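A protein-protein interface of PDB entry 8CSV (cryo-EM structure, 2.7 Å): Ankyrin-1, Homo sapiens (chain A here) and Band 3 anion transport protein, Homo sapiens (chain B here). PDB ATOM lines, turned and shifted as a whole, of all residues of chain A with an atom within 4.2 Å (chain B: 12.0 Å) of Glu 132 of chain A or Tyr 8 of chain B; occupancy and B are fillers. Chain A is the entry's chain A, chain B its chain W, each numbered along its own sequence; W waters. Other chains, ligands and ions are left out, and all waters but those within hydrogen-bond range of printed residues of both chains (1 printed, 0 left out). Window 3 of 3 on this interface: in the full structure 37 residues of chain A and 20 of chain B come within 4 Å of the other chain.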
ATOM      1  N   LYS A 128      21.839  -6.713  11.436  1.00  0.00           N
ATOM      2  CA  LYS A 128      22.276  -7.880  12.195  1.00  0.00           C
ATOM      3  C   LYS A 128      21.105  -8.555  12.895  1.00  0.00           C
ATOM      4  O   LYS A 128      20.973  -9.785  12.857  1.00  0.00           O
ATOM      5  CB  LYS A 128      23.337  -7.473  13.217  1.00  0.00           C
ATOM      6  CG  LYS A 128      24.653  -7.013  12.619  1.00  0.00           C
ATOM      7  CD  LYS A 128      25.527  -6.343  13.668  1.00  0.00           C
ATOM      8  CE  LYS A 128      25.712  -7.228  14.890  1.00  0.00           C
ATOM      9  NZ  LYS A 128      26.357  -8.525  14.548  1.00  0.00           N
ATOM     10  N   PHE A 129      20.235  -7.763  13.529  1.00  0.00           N
ATOM     11  CA  PHE A 129      19.101  -8.342  14.241  1.00  0.00           C
ATOM     12  C   PHE A 129      18.121  -9.009  13.283  1.00  0.00           C
ATOM     13  O   PHE A 129      17.599 -10.090  13.577  1.00  0.00           O
ATOM     14  CB  PHE A 129      18.397  -7.272  15.072  1.00  0.00           C
ATOM     15  CG  PHE A 129      17.317  -7.817  15.957  1.00  0.00           C
ATOM     16  CD1 PHE A 129      17.635  -8.437  17.154  1.00  0.00           C
ATOM     17  CD2 PHE A 129      15.987  -7.720  15.591  1.00  0.00           C
ATOM     18  CE1 PHE A 129      16.646  -8.946  17.968  1.00  0.00           C
ATOM     19  CE2 PHE A 129      14.995  -8.226  16.402  1.00  0.00           C
ATOM     20  CZ  PHE A 129      15.322  -8.839  17.591  1.00  0.00           C
ATOM     21  N   LEU A 130      17.853  -8.382  12.133  1.00  0.00           N
ATOM     22  CA  LEU A 130      16.926  -8.973  11.173  1.00  0.00           C
ATOM     23  C   LEU A 130      17.489 -10.255  10.573  1.00  0.00           C
ATOM     24  O   LEU A 130      16.753 -11.233  10.395  1.00  0.00           O
ATOM     25  CB  LEU A 130      16.589  -7.965  10.076  1.00  0.00           C
ATOM     26  CG  LEU A 130      15.674  -6.809  10.484  1.00  0.00           C
ATOM     27  CD1 LEU A 130      15.534  -5.819   9.346  1.00  0.00           C
ATOM     28  CD2 LEU A 130      14.311  -7.322  10.920  1.00  0.00           C
ATOM     29  N   LEU A 131      18.787 -10.274  10.259  1.00  0.00           N
ATOM     30  CA  LEU A 131      19.403 -11.493   9.743  1.00  0.00           C
ATOM     31  C   LEU A 131      19.384 -12.604  10.784  1.00  0.00           C
ATOM     32  O   LEU A 131      19.159 -13.772  10.450  1.00  0.00           O
ATOM     33  CB  LEU A 131      20.832 -11.208   9.283  1.00  0.00           C
ATOM     34  CG  LEU A 131      20.981 -10.437   7.972  1.00  0.00           C
ATOM     35  CD1 LEU A 131      22.425 -10.020   7.761  1.00  0.00           C
ATOM     36  CD2 LEU A 131      20.487 -11.273   6.804  1.00  0.00           C
ATOM     37  N   GLU A 132      19.617 -12.260  12.054  1.00  0.00           N
ATOM     38  CA  GLU A 132      19.548 -13.264  13.111  1.00  0.00           C
ATOM     39  C   GLU A 132      18.123 -13.772  13.306  1.00  0.00           C
ATOM     40  O   GLU A 132      17.917 -14.882  13.809  1.00  0.00           O
ATOM     41  CB  GLU A 132      20.087 -12.693  14.420  1.00  0.00           C
ATOM     42  CG  GLU A 132      21.593 -12.564  14.476  1.00  0.00           C
ATOM     43  CD  GLU A 132      22.057 -11.888  15.747  1.00  0.00           C
ATOM     44  OE1 GLU A 132      21.210 -11.283  16.436  1.00  0.00           O
ATOM     45  OE2 GLU A 132      23.264 -11.965  16.059  1.00  0.00           O
ATOM     46  N   ASN A 133      17.130 -12.976  12.922  1.00  0.00           N
ATOM     47  CA  ASN A 133      15.735 -13.352  13.111  1.00  0.00           C
ATOM     48  C   ASN A 133      15.091 -13.936  11.861  1.00  0.00           C
ATOM     49  O   ASN A 133      13.869 -14.112  11.844  1.00  0.00           O
ATOM     50  CB  ASN A 133      14.929 -12.149  13.604  1.00  0.00           C
ATOM     51  CG  ASN A 133      15.233 -11.806  15.046  1.00  0.00           C
ATOM     52  OD1 ASN A 133      14.563 -12.277  15.962  1.00  0.00           O
ATOM     53  ND2 ASN A 133      16.259 -10.996  15.256  1.00  0.00           N
ATOM     54  N   GLY A 134      15.868 -14.233  10.825  1.00  0.00           N
ATOM     55  CA  GLY A 134      15.367 -14.955   9.675  1.00  0.00           C
ATOM     56  C   GLY A 134      15.047 -14.131   8.448  1.00  0.00           C
ATOM     57  O   GLY A 134      14.394 -14.651   7.536  1.00  0.00           O
ATOM     58  N   TYR A 166      27.239 -13.295   6.590  1.00  0.00           N
ATOM     59  CA  TYR A 166      26.099 -14.041   7.115  1.00  0.00           C
ATOM     60  C   TYR A 166      25.538 -14.995   6.068  1.00  0.00           C
ATOM     61  O   TYR A 166      25.321 -16.180   6.346  1.00  0.00           O
ATOM     62  CB  TYR A 166      25.018 -13.076   7.605  1.00  0.00           C
ATOM     63  CG  TYR A 166      23.974 -13.724   8.486  1.00  0.00           C
ATOM     64  CD1 TYR A 166      22.849 -14.326   7.939  1.00  0.00           C
ATOM     65  CD2 TYR A 166      24.116 -13.735   9.866  1.00  0.00           C
ATOM     66  CE1 TYR A 166      21.897 -14.921   8.741  1.00  0.00           C
ATOM     67  CE2 TYR A 166      23.167 -14.324  10.677  1.00  0.00           C
ATOM     68  CZ  TYR A 166      22.062 -14.917  10.109  1.00  0.00           C
ATOM     69  OH  TYR A 166      21.115 -15.507  10.913  1.00  0.00           O
ATOM     70  N   LYS A 171      17.637 -18.588  10.589  1.00  0.00           N
ATOM     71  CA  LYS A 171      17.091 -18.200  11.885  1.00  0.00           C
ATOM     72  C   LYS A 171      17.889 -18.867  13.001  1.00  0.00           C
ATOM     73  O   LYS A 171      17.776 -20.078  13.217  1.00  0.00           O
ATOM     74  CB  LYS A 171      15.618 -18.588  11.957  1.00  0.00           C
ATOM     75  CG  LYS A 171      14.959 -18.367  13.306  1.00  0.00           C
ATOM     76  CD  LYS A 171      14.920 -16.900  13.674  1.00  0.00           C
ATOM     77  CE  LYS A 171      13.807 -16.612  14.665  1.00  0.00           C
ATOM     78  NZ  LYS A 171      12.473 -16.942  14.097  1.00  0.00           N
ATOM     79  N   VAL A 172      18.695 -18.079  13.711  1.00  0.00           N
ATOM     80  CA  VAL A 172      19.477 -18.593  14.830  1.00  0.00           C
ATOM     81  C   VAL A 172      18.787 -18.219  16.135  1.00  0.00           C
ATOM     82  O   VAL A 172      19.074 -18.795  17.190  1.00  0.00           O
ATOM     83  CB  VAL A 172      20.924 -18.067  14.794  1.00  0.00           C
ATOM     84  CG1 VAL A 172      21.642 -18.584  13.559  1.00  0.00           C
ATOM     85  CG2 VAL A 172      20.943 -16.548  14.826  1.00  0.00           C
ATOM     86  N   ARG A 173      17.876 -17.251  16.074  1.00  0.00           N
ATOM     87  CA  ARG A 173      17.097 -16.882  17.244  1.00  0.00           C
ATOM     88  C   ARG A 173      15.977 -17.887  17.488  1.00  0.00           C
ATOM     89  O   ARG A 173      15.543 -18.605  16.583  1.00  0.00           O
ATOM     90  CB  ARG A 173      16.504 -15.484  17.079  1.00  0.00           C
ATOM     91  CG  ARG A 173      17.485 -14.347  17.295  1.00  0.00           C
ATOM     92  CD  ARG A 173      17.010 -13.428  18.410  1.00  0.00           C
ATOM     93  NE  ARG A 173      15.623 -13.019  18.228  1.00  0.00           N
ATOM     94  CZ  ARG A 173      14.943 -12.267  19.082  1.00  0.00           C
ATOM     95  NH1 ARG A 173      15.495 -11.814  20.196  1.00  0.00           N
ATOM     96  NH2 ARG A 173      13.677 -11.963  18.814  1.00  0.00           N
ATOM     97  N   LEU A 174      15.513 -17.935  18.733  1.00  0.00           N
ATOM     98  CA  LEU A 174      14.351 -18.739  19.058  1.00  0.00           C
ATOM     99  C   LEU A 174      13.092 -18.100  18.475  1.00  0.00           C
ATOM    100  O   LEU A 174      13.069 -16.899  18.196  1.00  0.00           O
ATOM    101  CB  LEU A 174      14.199 -18.878  20.571  1.00  0.00           C
ATOM    102  CG  LEU A 174      15.169 -19.799  21.308  1.00  0.00           C
ATOM    103  CD1 LEU A 174      14.899 -19.744  22.799  1.00  0.00           C
ATOM    104  CD2 LEU A 174      15.044 -21.221  20.793  1.00  0.00           C
ATOM    105  N   GLU B   2      25.512  -8.114  26.972  1.00  0.00           N
ATOM    106  CA  GLU B   2      24.717  -9.142  26.312  1.00  0.00           C
ATOM    107  C   GLU B   2      23.382  -9.344  27.023  1.00  0.00           C
ATOM    108  O   GLU B   2      22.414  -8.633  26.751  1.00  0.00           O
ATOM    109  CB  GLU B   2      25.489 -10.463  26.256  1.00  0.00           C
ATOM    110  N   GLU B   3      23.346 -10.330  27.923  1.00  0.00           N
ATOM    111  CA  GLU B   3      22.171 -10.675  28.726  1.00  0.00           C
ATOM    112  C   GLU B   3      20.972 -11.072  27.869  1.00  0.00           C
ATOM    113  O   GLU B   3      19.827 -10.978  28.321  1.00  0.00           O
ATOM    114  CB  GLU B   3      21.787  -9.534  29.677  1.00  0.00           C
ATOM    115  N   LEU B   4      21.213 -11.521  26.633  1.00  0.00           N
ATOM    116  CA  LEU B   4      20.134 -11.957  25.755  1.00  0.00           C
ATOM    117  C   LEU B   4      20.490 -13.232  24.999  1.00  0.00           C
ATOM    118  O   LEU B   4      19.870 -13.523  23.968  1.00  0.00           O
ATOM    119  CB  LEU B   4      19.758 -10.856  24.755  1.00  0.00           C
ATOM    120  CG  LEU B   4      18.982  -9.658  25.303  1.00  0.00           C
ATOM    121  CD1 LEU B   4      18.726  -8.639  24.206  1.00  0.00           C
ATOM    122  CD2 LEU B   4      17.673 -10.113  25.929  1.00  0.00           C
ATOM    123  N   GLN B   5      21.473 -13.997  25.479  1.00  0.00           N
ATOM    124  CA  GLN B   5      21.852 -15.238  24.814  1.00  0.00           C
ATOM    125  C   GLN B   5      20.758 -16.294  24.890  1.00  0.00           C
ATOM    126  O   GLN B   5      20.728 -17.195  24.046  1.00  0.00           O
ATOM    127  CB  GLN B   5      23.146 -15.787  25.420  1.00  0.00           C
ATOM    128  N   ASP B   6      19.849 -16.191  25.863  1.00  0.00           N
ATOM    129  CA  ASP B   6      18.769 -17.160  26.009  1.00  0.00           C
ATOM    130  C   ASP B   6      17.764 -17.108  24.867  1.00  0.00           C
ATOM    131  O   ASP B   6      16.921 -18.005  24.769  1.00  0.00           O
ATOM    132  CB  ASP B   6      18.047 -16.941  27.341  1.00  0.00           C
ATOM    133  N   ASP B   7      17.822 -16.084  24.015  1.00  0.00           N
ATOM    134  CA  ASP B   7      16.929 -15.982  22.871  1.00  0.00           C
ATOM    135  C   ASP B   7      17.423 -16.758  21.657  1.00  0.00           C
ATOM    136  O   ASP B   7      16.728 -16.784  20.637  1.00  0.00           O
ATOM    137  CB  ASP B   7      16.736 -14.512  22.487  1.00  0.00           C
ATOM    138  CG  ASP B   7      16.315 -13.651  23.664  1.00  0.00           C
ATOM    139  OD1 ASP B   7      16.247 -14.174  24.795  1.00  0.00           O
ATOM    140  OD2 ASP B   7      16.054 -12.448  23.455  1.00  0.00           O
ATOM    141  N   TYR B   8      18.592 -17.384  21.737  1.00  0.00           N
ATOM    142  CA  TYR B   8      19.181 -18.082  20.605  1.00  0.00           C
ATOM    143  C   TYR B   8      19.040 -19.591  20.767  1.00  0.00           C
ATOM    144  O   TYR B   8      18.921 -20.108  21.881  1.00  0.00           O
ATOM    145  CB  TYR B   8      20.654 -17.702  20.443  1.00  0.00           C
ATOM    146  CG  TYR B   8      20.860 -16.248  20.080  1.00  0.00           C
ATOM    147  CD1 TYR B   8      20.958 -15.273  21.063  1.00  0.00           C
ATOM    148  CD2 TYR B   8      20.949 -15.850  18.753  1.00  0.00           C
ATOM    149  CE1 TYR B   8      21.142 -13.943  20.735  1.00  0.00           C
ATOM    150  CE2 TYR B   8      21.135 -14.522  18.415  1.00  0.00           C
ATOM    151  CZ  TYR B   8      21.231 -13.574  19.410  1.00  0.00           C
ATOM    152  OH  TYR B   8      21.416 -12.251  19.081  1.00  0.00           O
ATOM    153  N   GLU B   9      19.048 -20.292  19.630  1.00  0.00           N
ATOM    154  CA  GLU B   9      18.795 -21.730  19.627  1.00  0.00           C
ATOM    155  C   GLU B   9      19.886 -22.499  20.363  1.00  0.00           C
ATOM    156  O   GLU B   9      19.590 -23.426  21.126  1.00  0.00           O
ATOM    157  CB  GLU B   9      18.672 -22.237  18.190  1.00  0.00           C
ATOM    158  CG  GLU B   9      17.510 -21.652  17.405  1.00  0.00           C
ATOM    159  CD  GLU B   9      16.206 -22.383  17.650  1.00  0.00           C
ATOM    160  OE1 GLU B   9      16.204 -23.360  18.426  1.00  0.00           O
ATOM    161  OE2 GLU B   9      15.182 -21.981  17.059  1.00  0.00           O
ATOM    162  N   ASP B  10      21.152 -22.137  20.143  1.00  0.00           N
ATOM    163  CA  ASP B  10      22.252 -22.917  20.705  1.00  0.00           C
ATOM    164  C   ASP B  10      22.321 -22.784  22.222  1.00  0.00           C
ATOM    165  O   ASP B  10      22.480 -23.786  22.931  1.00  0.00           O
ATOM    166  CB  ASP B  10      23.572 -22.490  20.066  1.00  0.00           C
ATOM    167  CG  ASP B  10      23.630 -22.807  18.588  1.00  0.00           C
ATOM    168  OD1 ASP B  10      22.662 -23.404  18.074  1.00  0.00           O
ATOM    169  OD2 ASP B  10      24.640 -22.460  17.940  1.00  0.00           O
ATOM    170  N   MET B  11      22.204 -21.559  22.738  1.00  0.00           N
ATOM    171  CA  MET B  11      22.253 -21.365  24.183  1.00  0.00           C
ATOM    172  C   MET B  11      21.049 -21.999  24.868  1.00  0.00           C
ATOM    173  O   MET B  11      21.180 -22.578  25.952  1.00  0.00           O
ATOM    174  CB  MET B  11      22.341 -19.876  24.512  1.00  0.00           C
ATOM    175  CG  MET B  11      22.450 -19.572  25.997  1.00  0.00           C
ATOM    176  SD  MET B  11      23.885 -20.348  26.764  1.00  0.00           S
ATOM    177  CE  MET B  11      25.216 -19.610  25.818  1.00  0.00           C
ATOM    178  N   MET B  12      19.869 -21.907  24.249  1.00  0.00           N
ATOM    179  CA  MET B  12      18.690 -22.558  24.812  1.00  0.00           C
ATOM    180  C   MET B  12      18.840 -24.075  24.808  1.00  0.00           C
ATOM    181  O   MET B  12      18.435 -24.744  25.766  1.00  0.00           O
ATOM    182  CB  MET B  12      17.437 -22.139  24.045  1.00  0.00           C
ATOM    183  CG  MET B  12      16.154 -22.761  24.574  1.00  0.00           C
ATOM    184  SD  MET B  12      15.922 -22.492  26.343  1.00  0.00           S
ATOM    185  CE  MET B  12      15.771 -20.710  26.409  1.00  0.00           C
ATOM    186  N   GLU B  13      19.416 -24.634  23.741  1.00  0.00           N
ATOM    187  CA  GLU B  13      19.657 -26.072  23.693  1.00  0.00           C
ATOM    188  C   GLU B  13      20.641 -26.501  24.773  1.00  0.00           C
ATOM    189  O   GLU B  13      20.466 -27.552  25.403  1.00  0.00           O
ATOM    190  CB  GLU B  13      20.169 -26.473  22.309  1.00  0.00           C
ATOM    191  CG  GLU B  13      20.414 -27.964  22.144  1.00  0.00           C
ATOM    192  CD  GLU B  13      20.863 -28.332  20.742  1.00  0.00           C
ATOM    193  OE1 GLU B  13      20.983 -27.421  19.897  1.00  0.00           O
ATOM    194  OE2 GLU B  13      21.097 -29.532  20.487  1.00  0.00           O
ATOM    195  N   GLU B  14      21.686 -25.702  24.997  1.00  0.00           N
ATOM    196  CA  GLU B  14      22.629 -25.999  26.072  1.00  0.00           C
ATOM    197  C   GLU B  14      21.959 -25.907  27.439  1.00  0.00           C
ATOM    198  O   GLU B  14      22.250 -26.706  28.336  1.00  0.00           O
ATOM    199  CB  GLU B  14      23.827 -25.054  25.995  1.00  0.00           C
ATOM    200  CG  GLU B  14      24.733 -25.287  24.796  1.00  0.00           C
ATOM    201  CD  GLU B  14      25.583 -26.536  24.936  1.00  0.00           C
ATOM    202  OE1 GLU B  14      25.783 -27.000  26.079  1.00  0.00           O
ATOM    203  OE2 GLU B  14      26.053 -27.055  23.901  1.00  0.00           O
ATOM    204  N   ASN B  15      21.067 -24.930  27.619  1.00  0.00           N
ATOM    205  CA  ASN B  15      20.384 -24.769  28.900  1.00  0.00           C
ATOM    206  C   ASN B  15      19.411 -25.912  29.166  1.00  0.00           C
ATOM    207  O   ASN B  15      19.274 -26.361  30.310  1.00  0.00           O
ATOM    208  CB  ASN B  15      19.652 -23.429  28.940  1.00  0.00           C
ATOM    209  CG  ASN B  15      20.598 -22.250  29.000  1.00  0.00           C
ATOM    210  OD1 ASN B  15      21.679 -22.336  29.582  1.00  0.00           O
ATOM    211  ND2 ASN B  15      20.197 -21.137  28.397  1.00  0.00           N
ATOM    212  N   LEU B  16      18.724 -26.393  28.127  1.00  0.00           N
ATOM    213  CA  LEU B  16      17.719 -27.433  28.320  1.00  0.00           C
ATOM    214  C   LEU B  16      18.345 -28.769  28.703  1.00  0.00           C
ATOM    215  O   LEU B  16      17.667 -29.615  29.295  1.00  0.00           O
ATOM    216  CB  LEU B  16      16.865 -27.576  27.062  1.00  0.00           C
ATOM    217  CG  LEU B  16      15.880 -26.425  26.841  1.00  0.00           C
ATOM    218  CD1 LEU B  16      15.375 -26.406  25.410  1.00  0.00           C
ATOM    219  CD2 LEU B  16      14.721 -26.511  27.822  1.00  0.00           C
ATOM    220  N   GLU B  17      19.623 -28.972  28.371  1.00  0.00           N
ATOM    221  CA  GLU B  17      20.405 -30.129  28.814  1.00  0.00           C
ATOM    222  C   GLU B  17      19.755 -31.447  28.384  1.00  0.00           C
ATOM    223  O   GLU B  17      19.318 -32.256  29.205  1.00  0.00           O
ATOM    224  CB  GLU B  17      20.628 -30.089  30.330  1.00  0.00           C
ATOM    225  CG  GLU B  17      21.392 -28.867  30.812  1.00  0.00           C
ATOM    226  CD  GLU B  17      21.610 -28.865  32.312  1.00  0.00           C
ATOM    227  OE1 GLU B  17      21.279 -29.877  32.964  1.00  0.00           O
ATOM    228  OE2 GLU B  17      22.109 -27.849  32.840  1.00  0.00           O
ATOM    229  N   GLN B  18      19.694 -31.646  27.065  1.00  0.00           N
ATOM    230  CA  GLN B  18      19.100 -32.861  26.518  1.00  0.00           C
ATOM    231  C   GLN B  18      19.873 -34.115  26.913  1.00  0.00           C
ATOM    232  O   GLN B  18      19.305 -35.212  26.892  1.00  0.00           O
ATOM    233  CB  GLN B  18      19.020 -32.765  24.993  1.00  0.00           C
ATOM    234  CG  GLN B  18      18.363 -31.494  24.484  1.00  0.00           C
ATOM    235  CD  GLN B  18      18.313 -31.430  22.969  1.00  0.00           C
ATOM    236  OE1 GLN B  18      18.085 -30.368  22.389  1.00  0.00           O
ATOM    237  NE2 GLN B  18      18.525 -32.568  22.319  1.00  0.00           N
HETATM  238  O   HOH W   1      21.726 -19.840  17.697  1.00  0.00           O
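OD2 of Asp 7 of chain B lies within salt-bridge range of NH1 of Arg 173 of chain A (3.4 Å). O of Val 172 of chain A lies within hydrogen-bond range of N of Glu 9 of chain B. OE1 of Glu 132 of chain A sits at hydrogen-bond distance from OH of Tyr 8 of chain B. The backbone NH (N) of Leu 174 of chain A sits at hydrogen-bond distance from the backbone carbonyl oxygen (O) of Asp 7 of chain B, 2.5 Å away. O of Arg 173 of chain A sits close to OE2 of Glu 9 of chain B, 3.4 Å away.
The guanidinium group of Arg 173 of chain A sits at hydrogen-bond distance from the side-chain amide oxygen of Asn 133 of chain A (2.6 Å). O of Glu 132 of chain A is in hydrogen-bond range of N of Val 172 of chain A, at 3.3 Å. The backbone carbonyl oxygen (O) of Glu 132 of chain A is in hydrogen-bond range of the backbone NH (N) of Arg 173 of chain A (3.3 Å).
CA of Tyr 8 of chain B touches O of Val 172 of chain A, 3.5 Å away. CG of Arg 173 of chain A touches CE2 of Tyr 8 of chain B (3.8 Å). Leu 174 of chain A touches Asp 6 of chain B (CD1 to O, 3.3 Å). O of Tyr 8 of chain B touches CG of Leu 174 of chain A (3.8 Å). Glu 9 of chain B touches Leu 174 of chain A. Leu 174 of chain A touches Met 12 of chain B (CD1 to CB, 3.7 Å).
No residue of chain B comes within 4 Å of Lys 128 of chain A. No residue of chain B comes within 4 Å of Phe 129 of chain A. Glu 132 of chain A touches just one residue of chain B: Tyr 8 (2.8 Å). No residue of chain B comes within 4 Å of Asn 133 of chain A. No residue of chain B comes within 4 Å of Gly 134 of chain A. Lys 171 of chain A touches none of the printed residues of chain B. Leu 174 of chain A touches just these residues of chain B: Asp 6 (3.3 Å), Asp 7 (2.5 Å), Tyr 8 (3.8 Å), Glu 9 (3.4 Å) and Met 12 (3.7 Å). Of the printed residues of chain A, Asp 6 of chain B touches Leu 174 (3.3 Å). Tyr 8 of chain B touches just these residues of chain A: Glu 132, Val 172, Arg 173 and Leu 174. Of the printed residues of chain A, Met 12 of chain B touches Leu 174. The nearest residue of chain B that does not touch Glu 132 of chain A is Asp 7 of chain B (7.2 Å).
Of the 12 printed residues of chain A, 4 touch a printed residue of chain B. Printed residues of chain A that touch a printed residue of chain B: Glu 132, Val 172, Arg 173 and Leu 174. Hydrophobic or aromatic side chains of chain A that line the printed part of chain B: Val 172 and Leu 174. Hydrophobic or aromatic side chains of chain B within 4 Å of the printed part of chain A: Tyr 8 and Met 12.
Water W1 lies within hydrogen-bond range of O of Val 172 of chain A, N of Glu 9 of chain B and N of Asp 10 of chain B.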
